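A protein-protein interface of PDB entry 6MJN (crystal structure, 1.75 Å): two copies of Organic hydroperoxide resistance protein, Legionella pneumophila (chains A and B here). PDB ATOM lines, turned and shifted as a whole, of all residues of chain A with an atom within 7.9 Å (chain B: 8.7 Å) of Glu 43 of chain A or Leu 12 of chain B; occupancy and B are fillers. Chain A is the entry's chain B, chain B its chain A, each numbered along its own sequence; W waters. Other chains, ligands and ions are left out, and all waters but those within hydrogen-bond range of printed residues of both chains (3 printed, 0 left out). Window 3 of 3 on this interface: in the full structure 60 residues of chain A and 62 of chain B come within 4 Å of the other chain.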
ATOM      1  N   MET A  40      10.541  -0.406 -21.315  1.00  0.00           N
ATOM      2  CA  MET A  40       9.319   0.060 -20.689  1.00  0.00           C
ATOM      3  C   MET A  40       8.604   1.025 -21.632  1.00  0.00           C
ATOM      4  O   MET A  40       9.238   1.911 -22.212  1.00  0.00           O
ATOM      5  CB  MET A  40       9.614   0.755 -19.358  1.00  0.00           C
ATOM      6  CG  MET A  40       8.362   1.238 -18.626  1.00  0.00           C
ATOM      7  SD  MET A  40       8.651   1.662 -16.898  1.00  0.00           S
ATOM      8  CE  MET A  40       9.804   3.025 -17.057  1.00  0.00           C
ATOM      9  N   PRO A  41       7.298   0.877 -21.807  1.00  0.00           N
ATOM     10  CA  PRO A  41       6.582   1.735 -22.757  1.00  0.00           C
ATOM     11  C   PRO A  41       6.570   3.203 -22.349  1.00  0.00           C
ATOM     12  O   PRO A  41       6.675   3.555 -21.171  1.00  0.00           O
ATOM     13  CB  PRO A  41       5.164   1.150 -22.768  1.00  0.00           C
ATOM     14  CG  PRO A  41       5.069   0.302 -21.560  1.00  0.00           C
ATOM     15  CD  PRO A  41       6.449  -0.198 -21.273  1.00  0.00           C
ATOM     16  N   ARG A  42       6.419   4.057 -23.361  1.00  0.00           N
ATOM     17  CA  ARG A  42       6.322   5.493 -23.128  1.00  0.00           C
ATOM     18  C   ARG A  42       5.172   5.826 -22.189  1.00  0.00           C
ATOM     19  O   ARG A  42       5.275   6.765 -21.392  1.00  0.00           O
ATOM     20  CB  ARG A  42       6.148   6.229 -24.459  1.00  0.00           C
ATOM     21  CG  ARG A  42       7.279   6.020 -25.463  1.00  0.00           C
ATOM     22  CD  ARG A  42       7.569   7.300 -26.222  1.00  0.00           C
ATOM     23  NE  ARG A  42       8.184   8.309 -25.359  1.00  0.00           N
ATOM     24  CZ  ARG A  42       7.975   9.616 -25.474  1.00  0.00           C
ATOM     25  NH1 ARG A  42       7.155  10.079 -26.410  1.00  0.00           N
ATOM     26  NH2 ARG A  42       8.578  10.464 -24.646  1.00  0.00           N
ATOM     27  N   GLU A  43       4.080   5.058 -22.258  1.00  0.00           N
ATOM     28  CA  GLU A  43       2.912   5.333 -21.432  1.00  0.00           C
ATOM     29  C   GLU A  43       3.206   5.197 -19.947  1.00  0.00           C
ATOM     30  O   GLU A  43       2.460   5.740 -19.130  1.00  0.00           O
ATOM     31  CB  GLU A  43       1.759   4.399 -21.815  1.00  0.00           C
ATOM     32  CG  GLU A  43       1.148   4.672 -23.183  1.00  0.00           C
ATOM     33  CD  GLU A  43       1.792   3.861 -24.289  1.00  0.00           C
ATOM     34  OE1 GLU A  43       2.981   3.498 -24.155  1.00  0.00           O
ATOM     35  OE2 GLU A  43       1.102   3.574 -25.290  1.00  0.00           O
ATOM     36  N   LEU A  44       4.263   4.475 -19.576  1.00  0.00           N
ATOM     37  CA  LEU A  44       4.660   4.344 -18.182  1.00  0.00           C
ATOM     38  C   LEU A  44       5.933   5.124 -17.878  1.00  0.00           C
ATOM     39  O   LEU A  44       6.622   4.820 -16.899  1.00  0.00           O
ATOM     40  CB  LEU A  44       4.851   2.872 -17.811  1.00  0.00           C
ATOM     41  CG  LEU A  44       3.679   1.898 -17.993  1.00  0.00           C
ATOM     42  CD1 LEU A  44       4.094   0.478 -17.611  1.00  0.00           C
ATOM     43  CD2 LEU A  44       2.474   2.339 -17.180  1.00  0.00           C
ATOM     44  N   GLY A  45       6.272   6.108 -18.709  1.00  0.00           N
ATOM     45  CA  GLY A  45       7.480   6.875 -18.501  1.00  0.00           C
ATOM     46  C   GLY A  45       8.750   6.241 -19.021  1.00  0.00           C
ATOM     47  O   GLY A  45       9.837   6.754 -18.737  1.00  0.00           O
ATOM     48  N   GLY A  46       8.650   5.139 -19.771  1.00  0.00           N
ATOM     49  CA  GLY A  46       9.810   4.528 -20.386  1.00  0.00           C
ATOM     50  C   GLY A  46      10.144   5.148 -21.731  1.00  0.00           C
ATOM     51  O   GLY A  46       9.517   6.101 -22.194  1.00  0.00           O
ATOM     52  N   GLU A  47      11.163   4.579 -22.373  1.00  0.00           N
ATOM     53  CA  GLU A  47      11.612   5.067 -23.670  1.00  0.00           C
ATOM     54  C   GLU A  47      10.942   4.366 -24.849  1.00  0.00           C
ATOM     55  O   GLU A  47      11.040   4.867 -25.975  1.00  0.00           O
ATOM     56  CB  GLU A  47      13.135   4.923 -23.794  1.00  0.00           C
ATOM     57  N   GLY A  48      10.252   3.248 -24.622  1.00  0.00           N
ATOM     58  CA  GLY A  48       9.692   2.460 -25.708  1.00  0.00           C
ATOM     59  C   GLY A  48      10.776   1.983 -26.656  1.00  0.00           C
ATOM     60  O   GLY A  48      11.943   1.833 -26.287  1.00  0.00           O
ATOM     61  N   ASN A  52       7.625  -5.621 -24.800  1.00  0.00           N
ATOM     62  CA  ASN A  52       7.444  -5.711 -23.354  1.00  0.00           C
ATOM     63  C   ASN A  52       6.566  -6.927 -23.053  1.00  0.00           C
ATOM     64  O   ASN A  52       5.948  -7.503 -23.966  1.00  0.00           O
ATOM     65  CB  ASN A  52       6.813  -4.420 -22.795  1.00  0.00           C
ATOM     66  CG  ASN A  52       5.511  -4.074 -23.483  1.00  0.00           C
ATOM     67  OD1 ASN A  52       4.548  -4.813 -23.364  1.00  0.00           O
ATOM     68  ND2 ASN A  52       5.471  -2.934 -24.186  1.00  0.00           N
ATOM     69  N   GLN A  55       2.921  -6.992 -24.535  1.00  0.00           N
ATOM     70  CA  GLN A  55       2.883  -7.307 -25.960  1.00  0.00           C
ATOM     71  C   GLN A  55       3.101  -8.792 -26.199  1.00  0.00           C
ATOM     72  O   GLN A  55       2.458  -9.401 -27.064  1.00  0.00           O
ATOM     73  CB  GLN A  55       3.947  -6.490 -26.706  1.00  0.00           C
ATOM     74  CG  GLN A  55       3.591  -5.019 -26.792  1.00  0.00           C
ATOM     75  CD  GLN A  55       4.399  -4.253 -27.828  1.00  0.00           C
ATOM     76  OE1 GLN A  55       5.476  -4.683 -28.267  1.00  0.00           O
ATOM     77  NE2 GLN A  55       3.883  -3.098 -28.211  1.00  0.00           N
ATOM     78  N   SER A  90      -4.488  -4.985 -21.514  1.00  0.00           N
ATOM     79  CA  SER A  90      -4.288  -3.777 -20.733  1.00  0.00           C
ATOM     80  C   SER A  90      -3.702  -4.139 -19.375  1.00  0.00           C
ATOM     81  O   SER A  90      -3.989  -5.198 -18.810  1.00  0.00           O
ATOM     82  CB  SER A  90      -5.597  -3.002 -20.540  1.00  0.00           C
ATOM     83  OG  SER A  90      -6.013  -2.450 -21.765  1.00  0.00           O
ATOM     84  N   LEU A  91      -2.884  -3.234 -18.858  1.00  0.00           N
ATOM     85  CA  LEU A  91      -2.284  -3.377 -17.547  1.00  0.00           C
ATOM     86  C   LEU A  91      -3.034  -2.460 -16.587  1.00  0.00           C
ATOM     87  O   LEU A  91      -3.318  -1.298 -16.923  1.00  0.00           O
ATOM     88  CB  LEU A  91      -0.792  -3.033 -17.614  1.00  0.00           C
ATOM     89  CG  LEU A  91       0.006  -3.036 -16.309  1.00  0.00           C
ATOM     90  CD1 LEU A  91       0.134  -4.462 -15.775  1.00  0.00           C
ATOM     91  CD2 LEU A  91       1.384  -2.426 -16.543  1.00  0.00           C
ATOM     92  N   TYR A  92      -3.394  -2.990 -15.413  1.00  0.00           N
ATOM     93  CA  TYR A  92      -4.074  -2.203 -14.385  1.00  0.00           C
ATOM     94  C   TYR A  92      -3.356  -2.356 -13.049  1.00  0.00           C
ATOM     95  O   TYR A  92      -2.761  -3.399 -12.755  1.00  0.00           O
ATOM     96  CB  TYR A  92      -5.548  -2.636 -14.210  1.00  0.00           C
ATOM     97  CG  TYR A  92      -6.379  -2.603 -15.474  1.00  0.00           C
ATOM     98  CD1 TYR A  92      -6.446  -3.714 -16.318  1.00  0.00           C
ATOM     99  CD2 TYR A  92      -7.107  -1.468 -15.818  1.00  0.00           C
ATOM    100  CE1 TYR A  92      -7.220  -3.690 -17.481  1.00  0.00           C
ATOM    101  CE2 TYR A  92      -7.865  -1.422 -16.975  1.00  0.00           C
ATOM    102  CZ  TYR A  92      -7.921  -2.540 -17.804  1.00  0.00           C
ATOM    103  OH  TYR A  92      -8.679  -2.517 -18.955  1.00  0.00           O
ATOM    104  N   ALA A  93      -3.420  -1.311 -12.230  1.00  0.00           N
ATOM    105  CA  ALA A  93      -2.926  -1.384 -10.859  1.00  0.00           C
ATOM    106  C   ALA A  93      -3.988  -2.014  -9.963  1.00  0.00           C
ATOM    107  O   ALA A  93      -5.186  -1.783 -10.148  1.00  0.00           O
ATOM    108  CB  ALA A  93      -2.561   0.008 -10.330  1.00  0.00           C
ATOM    109  N   THR A  94      -3.523  -2.847  -8.945  1.00  0.00           N
ATOM    110  CA  THR A  94      -4.462  -3.451  -8.000  1.00  0.00           C
ATOM    111  C   THR A  94      -4.467  -2.719  -6.656  1.00  0.00           C
ATOM    112  O   THR A  94      -3.456  -2.137  -6.241  1.00  0.00           O
ATOM    113  CB  THR A  94      -4.112  -4.924  -7.751  1.00  0.00           C
ATOM    114  OG1 THR A  94      -2.898  -5.004  -6.993  1.00  0.00           O
ATOM    115  CG2 THR A  94      -3.953  -5.696  -9.060  1.00  0.00           C
ATOM    116  N   GLY A  98      -0.184  -4.541  -6.419  1.00  0.00           N
ATOM    117  CA  GLY A  98       0.303  -5.334  -7.518  1.00  0.00           C
ATOM    118  C   GLY A  98      -0.220  -4.848  -8.854  1.00  0.00           C
ATOM    119  O   GLY A  98      -0.694  -3.712  -8.998  1.00  0.00           O
ATOM    120  N   PHE A  99      -0.138  -5.724  -9.856  1.00  0.00           N
ATOM    121  CA  PHE A  99      -0.594  -5.410 -11.200  1.00  0.00           C
ATOM    122  C   PHE A  99      -1.446  -6.556 -11.716  1.00  0.00           C
ATOM    123  O   PHE A  99      -1.258  -7.706 -11.314  1.00  0.00           O
ATOM    124  CB  PHE A  99       0.584  -5.163 -12.142  1.00  0.00           C
ATOM    125  CG  PHE A  99       1.431  -3.991 -11.739  1.00  0.00           C
ATOM    126  CD1 PHE A  99       1.062  -2.701 -12.091  1.00  0.00           C
ATOM    127  CD2 PHE A  99       2.580  -4.176 -10.983  1.00  0.00           C
ATOM    128  CE1 PHE A  99       1.834  -1.614 -11.704  1.00  0.00           C
ATOM    129  CE2 PHE A  99       3.355  -3.090 -10.595  1.00  0.00           C
ATOM    130  CZ  PHE A  99       2.978  -1.812 -10.958  1.00  0.00           C
ATOM    131  N   LYS A 100      -2.394  -6.234 -12.599  1.00  0.00           N
ATOM    132  CA  LYS A 100      -3.215  -7.261 -13.228  1.00  0.00           C
ATOM    133  C   LYS A 100      -3.441  -6.936 -14.697  1.00  0.00           C
ATOM    134  O   LYS A 100      -3.328  -5.788 -15.136  1.00  0.00           O
ATOM    135  CB  LYS A 100      -4.580  -7.423 -12.524  1.00  0.00           C
ATOM    136  CG  LYS A 100      -5.550  -6.293 -12.768  1.00  0.00           C
ATOM    137  CD  LYS A 100      -6.903  -6.571 -12.106  1.00  0.00           C
ATOM    138  CE  LYS A 100      -7.823  -5.349 -12.150  1.00  0.00           C
ATOM    139  NZ  LYS A 100      -9.175  -5.624 -11.576  1.00  0.00           N
ATOM    140  N   LYS B  10      -8.590   3.049 -14.593  1.00  0.00           N
ATOM    141  CA  LYS B  10      -8.209   3.198 -15.997  1.00  0.00           C
ATOM    142  C   LYS B  10      -6.904   2.458 -16.278  1.00  0.00           C
ATOM    143  O   LYS B  10      -6.051   2.332 -15.396  1.00  0.00           O
ATOM    144  CB  LYS B  10      -8.069   4.678 -16.366  1.00  0.00           C
ATOM    145  N   ALA B  11      -6.756   1.979 -17.511  1.00  0.00           N
ATOM    146  CA  ALA B  11      -5.582   1.198 -17.881  1.00  0.00           C
ATOM    147  C   ALA B  11      -4.311   2.030 -17.762  1.00  0.00           C
ATOM    148  O   ALA B  11      -4.283   3.210 -18.125  1.00  0.00           O
ATOM    149  CB  ALA B  11      -5.729   0.669 -19.305  1.00  0.00           C
ATOM    150  N   LEU B  12      -3.253   1.411 -17.234  1.00  0.00           N
ATOM    151  CA  LEU B  12      -1.947   2.056 -17.259  1.00  0.00           C
ATOM    152  C   LEU B  12      -1.331   1.987 -18.651  1.00  0.00           C
ATOM    153  O   LEU B  12      -0.569   2.878 -19.039  1.00  0.00           O
ATOM    154  CB  LEU B  12      -1.015   1.409 -16.234  1.00  0.00           C
ATOM    155  CG  LEU B  12      -1.458   1.310 -14.769  1.00  0.00           C
ATOM    156  CD1 LEU B  12      -0.345   0.708 -13.922  1.00  0.00           C
ATOM    157  CD2 LEU B  12      -1.913   2.635 -14.214  1.00  0.00           C
ATOM    158  N   TYR B  13      -1.663   0.952 -19.419  1.00  0.00           N
ATOM    159  CA  TYR B  13      -1.023   0.688 -20.699  1.00  0.00           C
ATOM    160  C   TYR B  13      -1.891  -0.305 -21.451  1.00  0.00           C
ATOM    161  O   TYR B  13      -2.413  -1.245 -20.845  1.00  0.00           O
ATOM    162  CB  TYR B  13       0.392   0.120 -20.494  1.00  0.00           C
ATOM    163  CG  TYR B  13       1.074  -0.372 -21.755  1.00  0.00           C
ATOM    164  CD1 TYR B  13       1.443   0.512 -22.758  1.00  0.00           C
ATOM    165  CD2 TYR B  13       1.370  -1.717 -21.928  1.00  0.00           C
ATOM    166  CE1 TYR B  13       2.058   0.063 -23.922  1.00  0.00           C
ATOM    167  CE2 TYR B  13       1.980  -2.179 -23.090  1.00  0.00           C
ATOM    168  CZ  TYR B  13       2.334  -1.277 -24.077  1.00  0.00           C
ATOM    169  OH  TYR B  13       2.963  -1.721 -25.230  1.00  0.00           O
ATOM    170  N   THR B  14      -2.044  -0.097 -22.758  1.00  0.00           N
ATOM    171  CA  THR B  14      -2.842  -0.995 -23.585  1.00  0.00           C
ATOM    172  C   THR B  14      -2.091  -1.279 -24.874  1.00  0.00           C
ATOM    173  O   THR B  14      -1.478  -0.375 -25.452  1.00  0.00           O
ATOM    174  CB  THR B  14      -4.208  -0.371 -23.901  1.00  0.00           C
ATOM    175  OG1 THR B  14      -4.902  -0.107 -22.677  1.00  0.00           O
ATOM    176  CG2 THR B  14      -5.059  -1.288 -24.789  1.00  0.00           C
ATOM    177  N   THR B  15      -2.148  -2.532 -25.330  1.00  0.00           N
ATOM    178  CA  THR B  15      -1.493  -2.915 -26.565  1.00  0.00           C
ATOM    179  C   THR B  15      -2.364  -3.919 -27.309  1.00  0.00           C
ATOM    180  O   THR B  15      -3.159  -4.634 -26.707  1.00  0.00           O
ATOM    181  CB  THR B  15      -0.091  -3.495 -26.306  1.00  0.00           C
ATOM    182  OG1 THR B  15       0.552  -3.758 -27.561  1.00  0.00           O
ATOM    183  CG2 THR B  15      -0.166  -4.771 -25.489  1.00  0.00           C
ATOM    184  N   ASP B  31       1.633  -1.317 -33.133  1.00  0.00           N
ATOM    185  CA  ASP B  31       2.669  -0.298 -33.208  1.00  0.00           C
ATOM    186  C   ASP B  31       3.943  -0.800 -33.876  1.00  0.00           C
ATOM    187  O   ASP B  31       4.893  -0.026 -34.015  1.00  0.00           O
ATOM    188  CB  ASP B  31       2.981   0.272 -31.814  1.00  0.00           C
ATOM    189  CG  ASP B  31       3.552  -0.766 -30.838  1.00  0.00           C
ATOM    190  OD1 ASP B  31       3.811  -1.925 -31.226  1.00  0.00           O
ATOM    191  OD2 ASP B  31       3.748  -0.399 -29.660  1.00  0.00           O
ATOM    192  N   LEU B  33       6.276  -2.860 -32.877  1.00  0.00           N
ATOM    193  CA  LEU B  33       7.444  -3.178 -32.057  1.00  0.00           C
ATOM    194  C   LEU B  33       7.705  -4.681 -31.971  1.00  0.00           C
ATOM    195  O   LEU B  33       8.842  -5.093 -31.699  1.00  0.00           O
ATOM    196  CB  LEU B  33       7.270  -2.595 -30.647  1.00  0.00           C
ATOM    197  CG  LEU B  33       7.357  -1.067 -30.537  1.00  0.00           C
ATOM    198  CD1 LEU B  33       7.134  -0.620 -29.093  1.00  0.00           C
ATOM    199  CD2 LEU B  33       8.690  -0.563 -31.067  1.00  0.00           C
HETATM  200  O   HOH W   1       3.681   0.020 -26.922  1.00  0.00           O
HETATM  201  O   HOH W   2      -1.715   2.603 -23.644  1.00  0.00           O
HETATM  202  O   HOH W   3      -5.191   0.921 -13.288  1.00  0.00           O
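The side-chain carboxylate of Asp 31 of chain B sits at hydrogen-bond distance from the side-chain amide nitrogen of Gln 55 of chain A (3.1 Å).
OH of Tyr 13 of chain B sits at hydrogen-bond distance from ND2 of Asn 52 of chain A.
The side-chain hydroxyl (OG) of Ser 90 of chain A lies within hydrogen-bond range of the side-chain hydroxyl (OG1) of Thr 14 of chain B, at 2.7 Å.
The side-chain amide nitrogen (NE2) of Gln 55 of chain A lies within hydrogen-bond range of the side-chain hydroxyl (OH) of Tyr 13 of chain B (3.4 Å).
The backbone NH (N) of Leu 12 of chain B sits at hydrogen-bond distance from the backbone carbonyl oxygen (O) of Leu 91 of chain A (2.7 Å).
The backbone NH of Leu 91 of chain A sits at hydrogen-bond distance from the backbone carbonyl oxygen of Tyr 13 of chain B, at 2.9 Å.
The side-chain hydroxyl (OG1) of Thr 15 of chain B lies close to the side-chain amide nitrogen (NE2) of Gln 55 of chain A (3.5 Å).
Tyr 13 of chain B touches Pro 41 of chain A (CE1 to CB, 3.5 Å).
Leu 12 of chain B touches Glu 43 of chain A.
Glu 43 of chain A touches Tyr 13 of chain B.
O of Leu 12 of chain B touches CD2 of Leu 44 of chain A (3.6 Å).
Leu 33 of chain B touches Gln 55 of chain A.
Ala 11 of chain B touches Ser 90 of chain A.
Leu 91 of chain A touches Ala 11 of chain B (O to CA, 3.5 Å).
Lys 10 of chain B touches Tyr 92 of chain A.
Tyr 92 of chain A touches Ala 11 of chain B.
Leu 12 of chain B touches Phe 99 of chain A (CD1 to CE1, 3.9 Å).
No position is printed for both chains.
Of the 18 pairs that touch across the chains among the printed residues, none has its exchanged pair printed and touching as well.
Of chain B, only Leu 12 (3.9 Å) and Tyr 13 (3.6 Å) come within 4 Å of Glu 43 of chain A.
Leu 12 of chain B touches four residues of chain A.
Of the printed residues of chain A, Ala 11 of chain B touches Ser 90 (3.9 Å), Leu 91 (3.5 Å) and Tyr 92 (3.6 Å).
Of the printed residues of chain B, Pro 41 of chain A touches Tyr 13.
Printed residues of chain A within 4 Å of Thr 14 of chain B: Ser 90 (2.7 Å).
Of the printed residues of chain B, Phe 99 of chain A touches Leu 12 (3.9 Å).
Of the printed residues of chain A, Leu 33 of chain B touches Gln 55.
Of the printed residues of chain A, Thr 15 of chain B touches Gln 55.
Lys 100 of chain A touches none of the printed residues of chain B.
The nearest residue of chain A that does not touch Leu 12 of chain B is Ala 93 of chain A (4.05 Å).
The nearest printed residue of chain B that does not touch Asn 52 of chain A is Thr 15 of chain B (5.2 Å).
Water W1 lies within hydrogen-bond range of OH of Tyr 13 of chain B (2.5 Å), OD2 of Asp 31 of chain B (2.8 Å) and NE2 of Gln 55 of chain A (3.4 Å).
Water W3 lies within hydrogen-bond range of the backbone carbonyl oxygen (O) of Lys 10 of chain B (2.7 Å) and the backbone NH (N) of Ala 93 of chain A (3.0 Å).
Water W2 lies within hydrogen-bond range of N of Thr 14 of chain B (2.9 Å) and OE2 of Glu 43 of chain A (3.4 Å).
OD1 of Asp 31 of chain B lies within hydrogen-bond range of N of Leu 33 of chain B (3.1 Å).
The backbone NH of Tyr 92 of chain A is in hydrogen-bond range of the backbone carbonyl oxygen of Lys 100 of chain A (2.8 Å).
The backbone carbonyl oxygen of Pro 41 of chain A is in hydrogen-bond range of the backbone NH of Gly 46 of chain A.
The backbone NH (N) of Gln 55 of chain A sits at hydrogen-bond distance from the side-chain amide oxygen (OD1) of Asn 52 of chain A, at 3.0 Å.
Printed residues of chain A that touch a printed residue of chain B: Pro 41, Glu 43, Leu 44, Asn 52, Gln 55, Ser 90, Leu 91, Tyr 92 and Phe 99.
Hydrophobic or aromatic side chains of chain B that line the printed part of chain A: Ala 11, Leu 12, Tyr 13 and Leu 33.
Among the printed residues, 18 pairs touch across the chains.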
